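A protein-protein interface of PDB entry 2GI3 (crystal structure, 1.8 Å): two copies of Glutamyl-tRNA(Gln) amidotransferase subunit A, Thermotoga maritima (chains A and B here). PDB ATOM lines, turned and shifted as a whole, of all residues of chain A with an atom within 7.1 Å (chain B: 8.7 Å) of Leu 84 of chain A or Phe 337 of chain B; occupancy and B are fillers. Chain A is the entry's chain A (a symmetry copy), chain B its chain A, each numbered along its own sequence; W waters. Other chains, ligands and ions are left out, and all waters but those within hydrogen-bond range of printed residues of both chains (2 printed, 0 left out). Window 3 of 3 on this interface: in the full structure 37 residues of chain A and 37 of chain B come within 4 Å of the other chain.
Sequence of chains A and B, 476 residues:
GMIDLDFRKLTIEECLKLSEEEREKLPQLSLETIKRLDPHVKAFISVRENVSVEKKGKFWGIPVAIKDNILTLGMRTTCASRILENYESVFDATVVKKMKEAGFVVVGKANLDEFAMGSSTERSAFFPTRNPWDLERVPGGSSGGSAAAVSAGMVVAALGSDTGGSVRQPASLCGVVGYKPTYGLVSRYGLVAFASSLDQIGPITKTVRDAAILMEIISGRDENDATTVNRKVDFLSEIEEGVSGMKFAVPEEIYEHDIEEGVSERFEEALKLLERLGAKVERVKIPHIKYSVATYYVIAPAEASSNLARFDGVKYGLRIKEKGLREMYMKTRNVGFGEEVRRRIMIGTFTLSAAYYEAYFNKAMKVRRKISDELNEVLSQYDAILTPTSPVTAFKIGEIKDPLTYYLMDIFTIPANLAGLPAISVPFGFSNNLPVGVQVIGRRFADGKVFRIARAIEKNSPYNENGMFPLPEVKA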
ATOM      1  N   ASP A  68     -27.577 -23.204  15.738  1.00  0.00           N
ATOM      2  CA  ASP A  68     -26.497 -22.220  15.936  1.00  0.00           C
ATOM      3  C   ASP A  68     -25.075 -22.706  15.587  1.00  0.00           C
ATOM      4  O   ASP A  68     -24.094 -22.160  16.071  1.00  0.00           O
ATOM      5  CB  ASP A  68     -26.555 -21.625  17.351  1.00  0.00           C
ATOM      6  CG  ASP A  68     -25.991 -20.210  17.408  1.00  0.00           C
ATOM      7  OD1 ASP A  68     -25.928 -19.560  16.358  1.00  0.00           O
ATOM      8  OD2 ASP A  68     -25.602 -19.783  18.513  1.00  0.00           O
ATOM      9  N   LEU A  71     -23.917 -20.241  10.138  1.00  0.00           N
ATOM     10  CA  LEU A  71     -23.521 -18.828  10.170  1.00  0.00           C
ATOM     11  C   LEU A  71     -24.623 -17.923   9.648  1.00  0.00           C
ATOM     12  O   LEU A  71     -25.263 -18.222   8.646  1.00  0.00           O
ATOM     13  CB  LEU A  71     -22.241 -18.617   9.373  1.00  0.00           C
ATOM     14  CG  LEU A  71     -20.994 -19.390   9.817  1.00  0.00           C
ATOM     15  CD1 LEU A  71     -19.843 -19.110   8.893  1.00  0.00           C
ATOM     16  CD2 LEU A  71     -20.605 -19.061  11.265  1.00  0.00           C
ATOM     17  N   ARG A  76     -25.273 -13.592  16.358  1.00  0.00           N
ATOM     18  CA  ARG A  76     -24.050 -14.323  16.580  1.00  0.00           C
ATOM     19  C   ARG A  76     -24.273 -15.817  16.271  1.00  0.00           C
ATOM     20  O   ARG A  76     -25.418 -16.258  16.154  1.00  0.00           O
ATOM     21  CB  ARG A  76     -23.557 -14.104  17.988  1.00  0.00           C
ATOM     22  CG  ARG A  76     -24.507 -14.493  19.075  1.00  0.00           C
ATOM     23  CD  ARG A  76     -24.387 -13.557  20.285  1.00  0.00           C
ATOM     24  NE  ARG A  76     -25.490 -13.780  21.230  1.00  0.00           N
ATOM     25  CZ  ARG A  76     -25.490 -14.643  22.258  1.00  0.00           C
ATOM     26  NH1 ARG A  76     -24.429 -15.387  22.549  1.00  0.00           N
ATOM     27  NH2 ARG A  76     -26.571 -14.746  23.027  1.00  0.00           N
ATOM     28  N   THR A  77     -23.171 -16.542  16.063  1.00  0.00           N
ATOM     29  CA  THR A  77     -23.184 -17.985  15.869  1.00  0.00           C
ATOM     30  C   THR A  77     -22.231 -18.567  16.920  1.00  0.00           C
ATOM     31  O   THR A  77     -21.045 -18.407  16.842  1.00  0.00           O
ATOM     32  CB  THR A  77     -22.770 -18.344  14.435  1.00  0.00           C
ATOM     33  OG1 THR A  77     -23.644 -17.647  13.512  1.00  0.00           O
ATOM     34  CG2 THR A  77     -22.828 -19.861  14.208  1.00  0.00           C
ATOM     35  N   THR A  78     -22.775 -19.184  17.945  1.00  0.00           N
ATOM     36  CA  THR A  78     -21.978 -19.630  19.049  1.00  0.00           C
ATOM     37  C   THR A  78     -21.487 -21.054  18.924  1.00  0.00           C
ATOM     38  O   THR A  78     -20.598 -21.461  19.673  1.00  0.00           O
ATOM     39  CB  THR A  78     -22.759 -19.509  20.373  1.00  0.00           C
ATOM     40  OG1 THR A  78     -23.822 -20.468  20.381  1.00  0.00           O
ATOM     41  CG2 THR A  78     -23.298 -18.072  20.535  1.00  0.00           C
ATOM     42  N   CYS A  79     -22.121 -21.860  18.053  1.00  0.00           N
ATOM     43  CA  CYS A  79     -21.966 -23.334  18.103  1.00  0.00           C
ATOM     44  C   CYS A  79     -22.154 -23.946  19.498  1.00  0.00           C
ATOM     45  O   CYS A  79     -21.578 -24.985  19.810  1.00  0.00           O
ATOM     46  CB  CYS A  79     -20.615 -23.768  17.552  1.00  0.00           C
ATOM     47  SG  CYS A  79     -20.352 -23.281  15.899  1.00  0.00           S
ATOM     48  N   ALA A  80     -22.980 -23.287  20.329  1.00  0.00           N
ATOM     49  CA  ALA A  80     -23.217 -23.601  21.724  1.00  0.00           C
ATOM     50  C   ALA A  80     -21.927 -23.791  22.512  1.00  0.00           C
ATOM     51  O   ALA A  80     -21.825 -24.709  23.324  1.00  0.00           O
ATOM     52  CB  ALA A  80     -24.204 -24.847  21.916  1.00  0.00           C
ATOM     53  N   SER A  81     -20.937 -22.955  22.201  1.00  0.00           N
ATOM     54  CA  SER A  81     -19.634 -22.952  22.860  1.00  0.00           C
ATOM     55  C   SER A  81     -19.399 -21.620  23.557  1.00  0.00           C
ATOM     56  O   SER A  81     -19.681 -20.564  22.998  1.00  0.00           O
ATOM     57  CB  SER A  81     -18.518 -23.075  21.834  1.00  0.00           C
ATOM     58  OG  SER A  81     -17.268 -23.252  22.459  1.00  0.00           O
ATOM     59  N   ARG A  82     -18.803 -21.675  24.740  1.00  0.00           N
ATOM     60  CA  ARG A  82     -18.483 -20.456  25.461  1.00  0.00           C
ATOM     61  C   ARG A  82     -17.509 -19.592  24.689  1.00  0.00           C
ATOM     62  O   ARG A  82     -17.622 -18.365  24.684  1.00  0.00           O
ATOM     63  CB  ARG A  82     -17.906 -20.778  26.845  1.00  0.00           C
ATOM     64  CG  ARG A  82     -18.954 -21.223  27.820  1.00  0.00           C
ATOM     65  CD  ARG A  82     -19.753 -20.051  28.341  1.00  0.00           C
ATOM     66  NE  ARG A  82     -20.966 -20.499  29.017  1.00  0.00           N
ATOM     67  CZ  ARG A  82     -21.858 -19.686  29.579  1.00  0.00           C
ATOM     68  NH1 ARG A  82     -21.690 -18.367  29.537  1.00  0.00           N
ATOM     69  NH2 ARG A  82     -22.936 -20.194  30.173  1.00  0.00           N
ATOM     70  N   ILE A  83     -16.568 -20.219  23.999  1.00  0.00           N
ATOM     71  CA  ILE A  83     -15.557 -19.445  23.301  1.00  0.00           C
ATOM     72  C   ILE A  83     -16.127 -18.594  22.163  1.00  0.00           C
ATOM     73  O   ILE A  83     -15.497 -17.597  21.755  1.00  0.00           O
ATOM     74  CB  ILE A  83     -14.385 -20.328  22.787  1.00  0.00           C
ATOM     75  CG1 ILE A  83     -13.172 -19.467  22.346  1.00  0.00           C
ATOM     76  CG2 ILE A  83     -14.834 -21.222  21.665  1.00  0.00           C
ATOM     77  CD1 ILE A  83     -12.584 -18.542  23.438  1.00  0.00           C
ATOM     78  N   LEU A  84     -17.308 -18.970  21.655  1.00  0.00           N
ATOM     79  CA  LEU A  84     -17.908 -18.257  20.541  1.00  0.00           C
ATOM     80  C   LEU A  84     -19.137 -17.500  21.020  1.00  0.00           C
ATOM     81  O   LEU A  84     -19.961 -17.019  20.232  1.00  0.00           O
ATOM     82  CB  LEU A  84     -18.223 -19.221  19.378  1.00  0.00           C
ATOM     83  CG  LEU A  84     -17.051 -19.827  18.580  1.00  0.00           C
ATOM     84  CD1 LEU A  84     -17.565 -20.675  17.391  1.00  0.00           C
ATOM     85  CD2 LEU A  84     -16.003 -18.810  18.096  1.00  0.00           C
ATOM     86  N   GLU A  85     -19.230 -17.311  22.324  1.00  0.00           N
ATOM     87  CA  GLU A  85     -20.391 -16.640  22.874  1.00  0.00           C
ATOM     88  C   GLU A  85     -20.663 -15.305  22.216  1.00  0.00           C
ATOM     89  O   GLU A  85     -21.797 -14.895  22.152  1.00  0.00           O
ATOM     90  CB  GLU A  85     -20.150 -16.305  24.334  1.00  0.00           C
ATOM     91  CG  GLU A  85     -20.461 -17.348  25.293  1.00  0.00           C
ATOM     92  CD  GLU A  85     -20.123 -16.895  26.692  1.00  0.00           C
ATOM     93  OE1 GLU A  85     -18.942 -16.572  26.963  1.00  0.00           O
ATOM     94  OE2 GLU A  85     -21.058 -16.834  27.506  1.00  0.00           O
ATOM     95  N   ASN A  86     -19.615 -14.592  21.783  1.00  0.00           N
ATOM     96  CA  ASN A  86     -19.809 -13.289  21.189  1.00  0.00           C
ATOM     97  C   ASN A  86     -19.362 -13.232  19.736  1.00  0.00           C
ATOM     98  O   ASN A  86     -19.177 -12.153  19.204  1.00  0.00           O
ATOM     99  CB  ASN A  86     -19.133 -12.211  22.044  1.00  0.00           C
ATOM    100  CG  ASN A  86     -19.886 -11.938  23.329  1.00  0.00           C
ATOM    101  OD1 ASN A  86     -21.021 -11.451  23.307  1.00  0.00           O
ATOM    102  ND2 ASN A  86     -19.248 -12.232  24.454  1.00  0.00           N
ATOM    103  N   TYR A  87     -19.233 -14.399  19.076  1.00  0.00           N
ATOM    104  CA  TYR A  87     -18.806 -14.453  17.703  1.00  0.00           C
ATOM    105  C   TYR A  87     -19.893 -14.022  16.697  1.00  0.00           C
ATOM    106  O   TYR A  87     -21.005 -14.524  16.710  1.00  0.00           O
ATOM    107  CB  TYR A  87     -18.278 -15.877  17.337  1.00  0.00           C
ATOM    108  CG  TYR A  87     -17.869 -15.946  15.919  1.00  0.00           C
ATOM    109  CD1 TYR A  87     -16.647 -15.430  15.520  1.00  0.00           C
ATOM    110  CD2 TYR A  87     -18.727 -16.465  14.936  1.00  0.00           C
ATOM    111  CE1 TYR A  87     -16.298 -15.415  14.223  1.00  0.00           C
ATOM    112  CE2 TYR A  87     -18.370 -16.450  13.631  1.00  0.00           C
ATOM    113  CZ  TYR A  87     -17.155 -15.923  13.284  1.00  0.00           C
ATOM    114  OH  TYR A  87     -16.776 -15.899  11.976  1.00  0.00           O
ATOM    115  N   GLU A  88     -19.521 -13.127  15.793  1.00  0.00           N
ATOM    116  CA  GLU A  88     -20.387 -12.677  14.714  1.00  0.00           C
ATOM    117  C   GLU A  88     -19.741 -13.004  13.395  1.00  0.00           C
ATOM    118  O   GLU A  88     -18.636 -12.563  13.128  1.00  0.00           O
ATOM    119  CB  GLU A  88     -20.603 -11.176  14.820  1.00  0.00           C
ATOM    120  CG  GLU A  88     -21.337 -10.775  16.094  1.00  0.00           C
ATOM    121  CD  GLU A  88     -22.813 -10.548  15.876  1.00  0.00           C
ATOM    122  OE1 GLU A  88     -23.273 -10.857  14.759  1.00  0.00           O
ATOM    123  OE2 GLU A  88     -23.510 -10.074  16.823  1.00  0.00           O
ATOM    124  N   PHE A 115     -20.559 -27.621  19.442  1.00  0.00           N
ATOM    125  CA  PHE A 115     -19.926 -27.991  18.165  1.00  0.00           C
ATOM    126  C   PHE A 115     -20.631 -29.172  17.457  1.00  0.00           C
ATOM    127  O   PHE A 115     -20.039 -29.843  16.584  1.00  0.00           O
ATOM    128  CB  PHE A 115     -18.413 -28.243  18.343  1.00  0.00           C
ATOM    129  CG  PHE A 115     -17.615 -26.992  18.696  1.00  0.00           C
ATOM    130  CD1 PHE A 115     -17.686 -25.865  17.914  1.00  0.00           C
ATOM    131  CD2 PHE A 115     -16.777 -26.975  19.797  1.00  0.00           C
ATOM    132  CE1 PHE A 115     -16.964 -24.709  18.241  1.00  0.00           C
ATOM    133  CE2 PHE A 115     -16.045 -25.828  20.118  1.00  0.00           C
ATOM    134  CZ  PHE A 115     -16.154 -24.699  19.350  1.00  0.00           C
ATOM    135  N   PHE A 126     -24.307 -23.785  27.195  1.00  0.00           N
ATOM    136  CA  PHE A 126     -25.188 -22.834  27.834  1.00  0.00           C
ATOM    137  C   PHE A 126     -26.246 -23.471  28.744  1.00  0.00           C
ATOM    138  O   PHE A 126     -26.376 -23.090  29.903  1.00  0.00           O
ATOM    139  CB  PHE A 126     -25.795 -21.917  26.766  1.00  0.00           C
ATOM    140  CG  PHE A 126     -24.752 -21.201  25.927  1.00  0.00           C
ATOM    141  CD1 PHE A 126     -23.767 -20.442  26.525  1.00  0.00           C
ATOM    142  CD2 PHE A 126     -24.749 -21.280  24.549  1.00  0.00           C
ATOM    143  CE1 PHE A 126     -22.802 -19.804  25.773  1.00  0.00           C
ATOM    144  CE2 PHE A 126     -23.779 -20.638  23.805  1.00  0.00           C
ATOM    145  CZ  PHE A 126     -22.820 -19.901  24.406  1.00  0.00           C
ATOM    146  N   VAL A 192     -20.573 -24.829  10.449  1.00  0.00           N
ATOM    147  CA  VAL A 192     -19.348 -25.044  11.227  1.00  0.00           C
ATOM    148  C   VAL A 192     -19.369 -26.543  11.578  1.00  0.00           C
ATOM    149  O   VAL A 192     -20.080 -26.958  12.457  1.00  0.00           O
ATOM    150  CB  VAL A 192     -19.262 -24.134  12.479  1.00  0.00           C
ATOM    151  CG1 VAL A 192     -17.911 -24.326  13.194  1.00  0.00           C
ATOM    152  CG2 VAL A 192     -19.406 -22.675  12.108  1.00  0.00           C
ATOM    153  N   PHE A 194     -17.404 -30.673  11.354  1.00  0.00           N
ATOM    154  CA  PHE A 194     -16.109 -31.396  11.489  1.00  0.00           C
ATOM    155  C   PHE A 194     -15.972 -32.703  10.644  1.00  0.00           C
ATOM    156  O   PHE A 194     -14.916 -33.381  10.722  1.00  0.00           O
ATOM    157  CB  PHE A 194     -15.804 -31.623  12.984  1.00  0.00           C
ATOM    158  CG  PHE A 194     -15.629 -30.324  13.783  1.00  0.00           C
ATOM    159  CD1 PHE A 194     -16.740 -29.532  14.125  1.00  0.00           C
ATOM    160  CD2 PHE A 194     -14.354 -29.895  14.190  1.00  0.00           C
ATOM    161  CE1 PHE A 194     -16.583 -28.345  14.857  1.00  0.00           C
ATOM    162  CE2 PHE A 194     -14.187 -28.705  14.927  1.00  0.00           C
ATOM    163  CZ  PHE A 194     -15.297 -27.930  15.260  1.00  0.00           C
ATOM    164  N   ASN B 334      -7.623 -11.873  22.431  1.00  0.00           N
ATOM    165  CA  ASN B 334      -8.455 -12.406  21.336  1.00  0.00           C
ATOM    166  C   ASN B 334      -8.002 -13.799  20.844  1.00  0.00           C
ATOM    167  O   ASN B 334      -7.691 -13.996  19.657  1.00  0.00           O
ATOM    168  CB  ASN B 334      -8.520 -11.416  20.169  1.00  0.00           C
ATOM    169  CG  ASN B 334      -9.531 -11.831  19.118  1.00  0.00           C
ATOM    170  OD1 ASN B 334      -9.200 -11.955  17.927  1.00  0.00           O
ATOM    171  ND2 ASN B 334     -10.763 -12.086  19.563  1.00  0.00           N
ATOM    172  N   VAL B 335      -7.989 -14.752  21.776  1.00  0.00           N
ATOM    173  CA  VAL B 335      -7.383 -16.074  21.568  1.00  0.00           C
ATOM    174  C   VAL B 335      -8.206 -17.162  22.274  1.00  0.00           C
ATOM    175  O   VAL B 335      -8.976 -16.867  23.199  1.00  0.00           O
ATOM    176  CB  VAL B 335      -5.901 -16.083  22.102  1.00  0.00           C
ATOM    177  CG1 VAL B 335      -5.328 -17.498  22.181  1.00  0.00           C
ATOM    178  CG2 VAL B 335      -5.009 -15.200  21.231  1.00  0.00           C
ATOM    179  N   GLY B 336      -8.045 -18.409  21.821  1.00  0.00           N
ATOM    180  CA  GLY B 336      -8.529 -19.580  22.562  1.00  0.00           C
ATOM    181  C   GLY B 336      -9.452 -20.516  21.802  1.00  0.00           C
ATOM    182  O   GLY B 336      -9.871 -21.541  22.350  1.00  0.00           O
ATOM    183  N   PHE B 337      -9.777 -20.184  20.552  1.00  0.00           N
ATOM    184  CA  PHE B 337     -10.650 -21.047  19.764  1.00  0.00           C
ATOM    185  C   PHE B 337     -10.017 -22.437  19.547  1.00  0.00           C
ATOM    186  O   PHE B 337     -10.692 -23.454  19.671  1.00  0.00           O
ATOM    187  CB  PHE B 337     -10.996 -20.405  18.426  1.00  0.00           C
ATOM    188  CG  PHE B 337     -11.930 -21.229  17.602  1.00  0.00           C
ATOM    189  CD1 PHE B 337     -13.241 -21.404  18.000  1.00  0.00           C
ATOM    190  CD2 PHE B 337     -11.499 -21.850  16.450  1.00  0.00           C
ATOM    191  CE1 PHE B 337     -14.128 -22.182  17.248  1.00  0.00           C
ATOM    192  CE2 PHE B 337     -12.375 -22.628  15.688  1.00  0.00           C
ATOM    193  CZ  PHE B 337     -13.702 -22.791  16.096  1.00  0.00           C
ATOM    194  N   GLY B 338      -8.727 -22.463  19.224  1.00  0.00           N
ATOM    195  CA  GLY B 338      -7.998 -23.714  19.048  1.00  0.00           C
ATOM    196  C   GLY B 338      -8.005 -24.591  20.287  1.00  0.00           C
ATOM    197  O   GLY B 338      -8.298 -25.784  20.197  1.00  0.00           O
ATOM    198  N   GLU B 339      -7.691 -24.002  21.443  1.00  0.00           N
ATOM    199  CA  GLU B 339      -7.621 -24.765  22.705  1.00  0.00           C
ATOM    200  C   GLU B 339      -8.956 -25.391  23.084  1.00  0.00           C
ATOM    201  O   GLU B 339      -8.987 -26.532  23.544  1.00  0.00           O
ATOM    202  CB  GLU B 339      -7.131 -23.898  23.867  1.00  0.00           C
ATOM    203  N   GLU B 340     -10.046 -24.649  22.896  1.00  0.00           N
ATOM    204  CA  GLU B 340     -11.380 -25.141  23.246  1.00  0.00           C
ATOM    205  C   GLU B 340     -11.794 -26.294  22.328  1.00  0.00           C
ATOM    206  O   GLU B 340     -12.419 -27.274  22.778  1.00  0.00           O
ATOM    207  CB  GLU B 340     -12.436 -24.008  23.167  1.00  0.00           C
ATOM    208  CG  GLU B 340     -13.916 -24.460  23.329  1.00  0.00           C
ATOM    209  CD  GLU B 340     -14.191 -25.230  24.641  1.00  0.00           C
ATOM    210  OE1 GLU B 340     -13.362 -25.160  25.569  1.00  0.00           O
ATOM    211  OE2 GLU B 340     -15.239 -25.915  24.744  1.00  0.00           O
ATOM    212  N   VAL B 341     -11.473 -26.157  21.041  1.00  0.00           N
ATOM    213  CA  VAL B 341     -11.821 -27.179  20.074  1.00  0.00           C
ATOM    214  C   VAL B 341     -11.016 -28.439  20.383  1.00  0.00           C
ATOM    215  O   VAL B 341     -11.563 -29.531  20.356  1.00  0.00           O
ATOM    216  CB  VAL B 341     -11.559 -26.727  18.630  1.00  0.00           C
ATOM    217  CG1 VAL B 341     -11.783 -27.894  17.680  1.00  0.00           C
ATOM    218  CG2 VAL B 341     -12.460 -25.540  18.260  1.00  0.00           C
ATOM    219  N   ARG B 342      -9.726 -28.282  20.683  1.00  0.00           N
ATOM    220  CA  ARG B 342      -8.881 -29.424  21.041  1.00  0.00           C
ATOM    221  C   ARG B 342      -9.387 -30.096  22.326  1.00  0.00           C
ATOM    222  O   ARG B 342      -9.480 -31.321  22.397  1.00  0.00           O
ATOM    223  CB  ARG B 342      -7.416 -28.999  21.187  1.00  0.00           C
ATOM    224  CG  ARG B 342      -6.444 -30.178  21.352  1.00  0.00           C
ATOM    225  CD  ARG B 342      -4.988 -29.801  21.064  1.00  0.00           C
ATOM    226  NE  ARG B 342      -4.766 -29.405  19.662  1.00  0.00           N
ATOM    227  CZ  ARG B 342      -4.673 -28.148  19.206  1.00  0.00           C
ATOM    228  NH1 ARG B 342      -4.783 -27.095  20.020  1.00  0.00           N
ATOM    229  NH2 ARG B 342      -4.473 -27.937  17.908  1.00  0.00           N
ATOM    230  N   ARG B 343      -9.724 -29.286  23.327  1.00  0.00           N
ATOM    231  CA  ARG B 343     -10.316 -29.778  24.569  1.00  0.00           C
ATOM    232  C   ARG B 343     -11.558 -30.603  24.315  1.00  0.00           C
ATOM    233  O   ARG B 343     -11.685 -31.708  24.833  1.00  0.00           O
ATOM    234  CB  ARG B 343     -10.723 -28.614  25.480  1.00  0.00           C
ATOM    235  CG  ARG B 343      -9.602 -28.029  26.307  1.00  0.00           C
ATOM    236  CD  ARG B 343     -10.151 -26.963  27.282  1.00  0.00           C
ATOM    237  NE  ARG B 343      -9.146 -25.933  27.544  1.00  0.00           N
ATOM    238  CZ  ARG B 343      -8.107 -26.073  28.367  1.00  0.00           C
ATOM    239  NH1 ARG B 343      -7.909 -27.210  29.036  1.00  0.00           N
ATOM    240  NH2 ARG B 343      -7.249 -25.069  28.519  1.00  0.00           N
ATOM    241  N   ARG B 344     -12.488 -30.049  23.546  1.00  0.00           N
ATOM    242  CA  ARG B 344     -13.745 -30.736  23.294  1.00  0.00           C
ATOM    243  C   ARG B 344     -13.481 -32.061  22.588  1.00  0.00           C
ATOM    244  O   ARG B 344     -14.060 -33.090  22.941  1.00  0.00           O
ATOM    245  CB  ARG B 344     -14.743 -29.873  22.497  1.00  0.00           C
ATOM    246  CG  ARG B 344     -15.603 -28.925  23.351  1.00  0.00           C
ATOM    247  CD  ARG B 344     -16.523 -29.655  24.381  1.00  0.00           C
ATOM    248  NE  ARG B 344     -17.427 -30.675  23.802  1.00  0.00           N
ATOM    249  CZ  ARG B 344     -17.272 -32.007  23.879  1.00  0.00           C
ATOM    250  NH1 ARG B 344     -16.243 -32.551  24.516  1.00  0.00           N
ATOM    251  NH2 ARG B 344     -18.158 -32.821  23.313  1.00  0.00           N
HETATM  252  O   HOH W   1     -15.696 -22.567  24.886  1.00  0.00           O
HETATM  253  O   HOH W   2     -17.776 -24.133  26.010  1.00  0.00           O
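Of chain B, only Phe 337 (3.8 Å) comes within 4 Å of Leu 84 of chain A.
Phe 337 of chain B touches three residues of chain A.
Gly 336 of chain B touches one residue of chain A.
Of the printed residues of chain A, Glu 340 of chain B touches Ser 81 (3.7 Å) and Ile 83 (3.8 Å).
Of the printed residues of chain B, Phe 115 of chain A touches Phe 337 and Val 341.
Of the printed residues of chain B, Ser 81 of chain A touches Glu 340 (3.7 Å).
The backbone carbonyl oxygen (O) of Cys 79 of chain A is in hydrogen-bond range of the backbone NH (N) of Phe 115 of chain A (2.8 Å).
The backbone NH of Ile 83 of chain A lies close to the side-chain hydroxyl of Ser 81 of chain A (3.5 Å).
Among the printed residues, pairs that only touch across the chains: Ser 81 of chain A with Glu 340 of chain B (3.7 Å), Ile 83 of chain A with Val 335 of chain B (3.99 Å), Ile 83 of chain A with Gly 336 of chain B (3.9 Å), Ile 83 of chain A with Phe 337 of chain B (3.9 Å), Ile 83 of chain A with Glu 340 of chain B (3.8 Å), Leu 84 of chain A with Phe 337 of chain B (3.8 Å), Phe 115 of chain A with Phe 337 of chain B (3.9 Å), Phe 115 of chain A with Val 341 of chain B (3.9 Å) and Phe 194 of chain A with Val 341 of chain B (3.7 Å).
Hydrophobic or aromatic side chains of chain B that line the printed part of chain A: Phe 337 and Val 341.
Of the 19 printed residues of chain A, 5 touch a printed residue of chain B.
Printed residues of chain A that touch a printed residue of chain B: Ser 81, Ile 83, Leu 84, Phe 115 and Phe 194.
Among the printed residues, 9 pairs touch across the chains.
No position is printed for both chains.
Water W1 lies within hydrogen-bond range of N of Ile 83 of chain A (2.7 Å), OG of Ser 81 of chain A (3.0 Å), N of Arg 82 of chain A (3.2 Å) and OE2 of Glu 340 of chain B (3.4 Å).
Water W2 bridges N of Arg 82 of chain A (3.0 Å) and OE2 of Glu 340 of chain B (3.3 Å).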
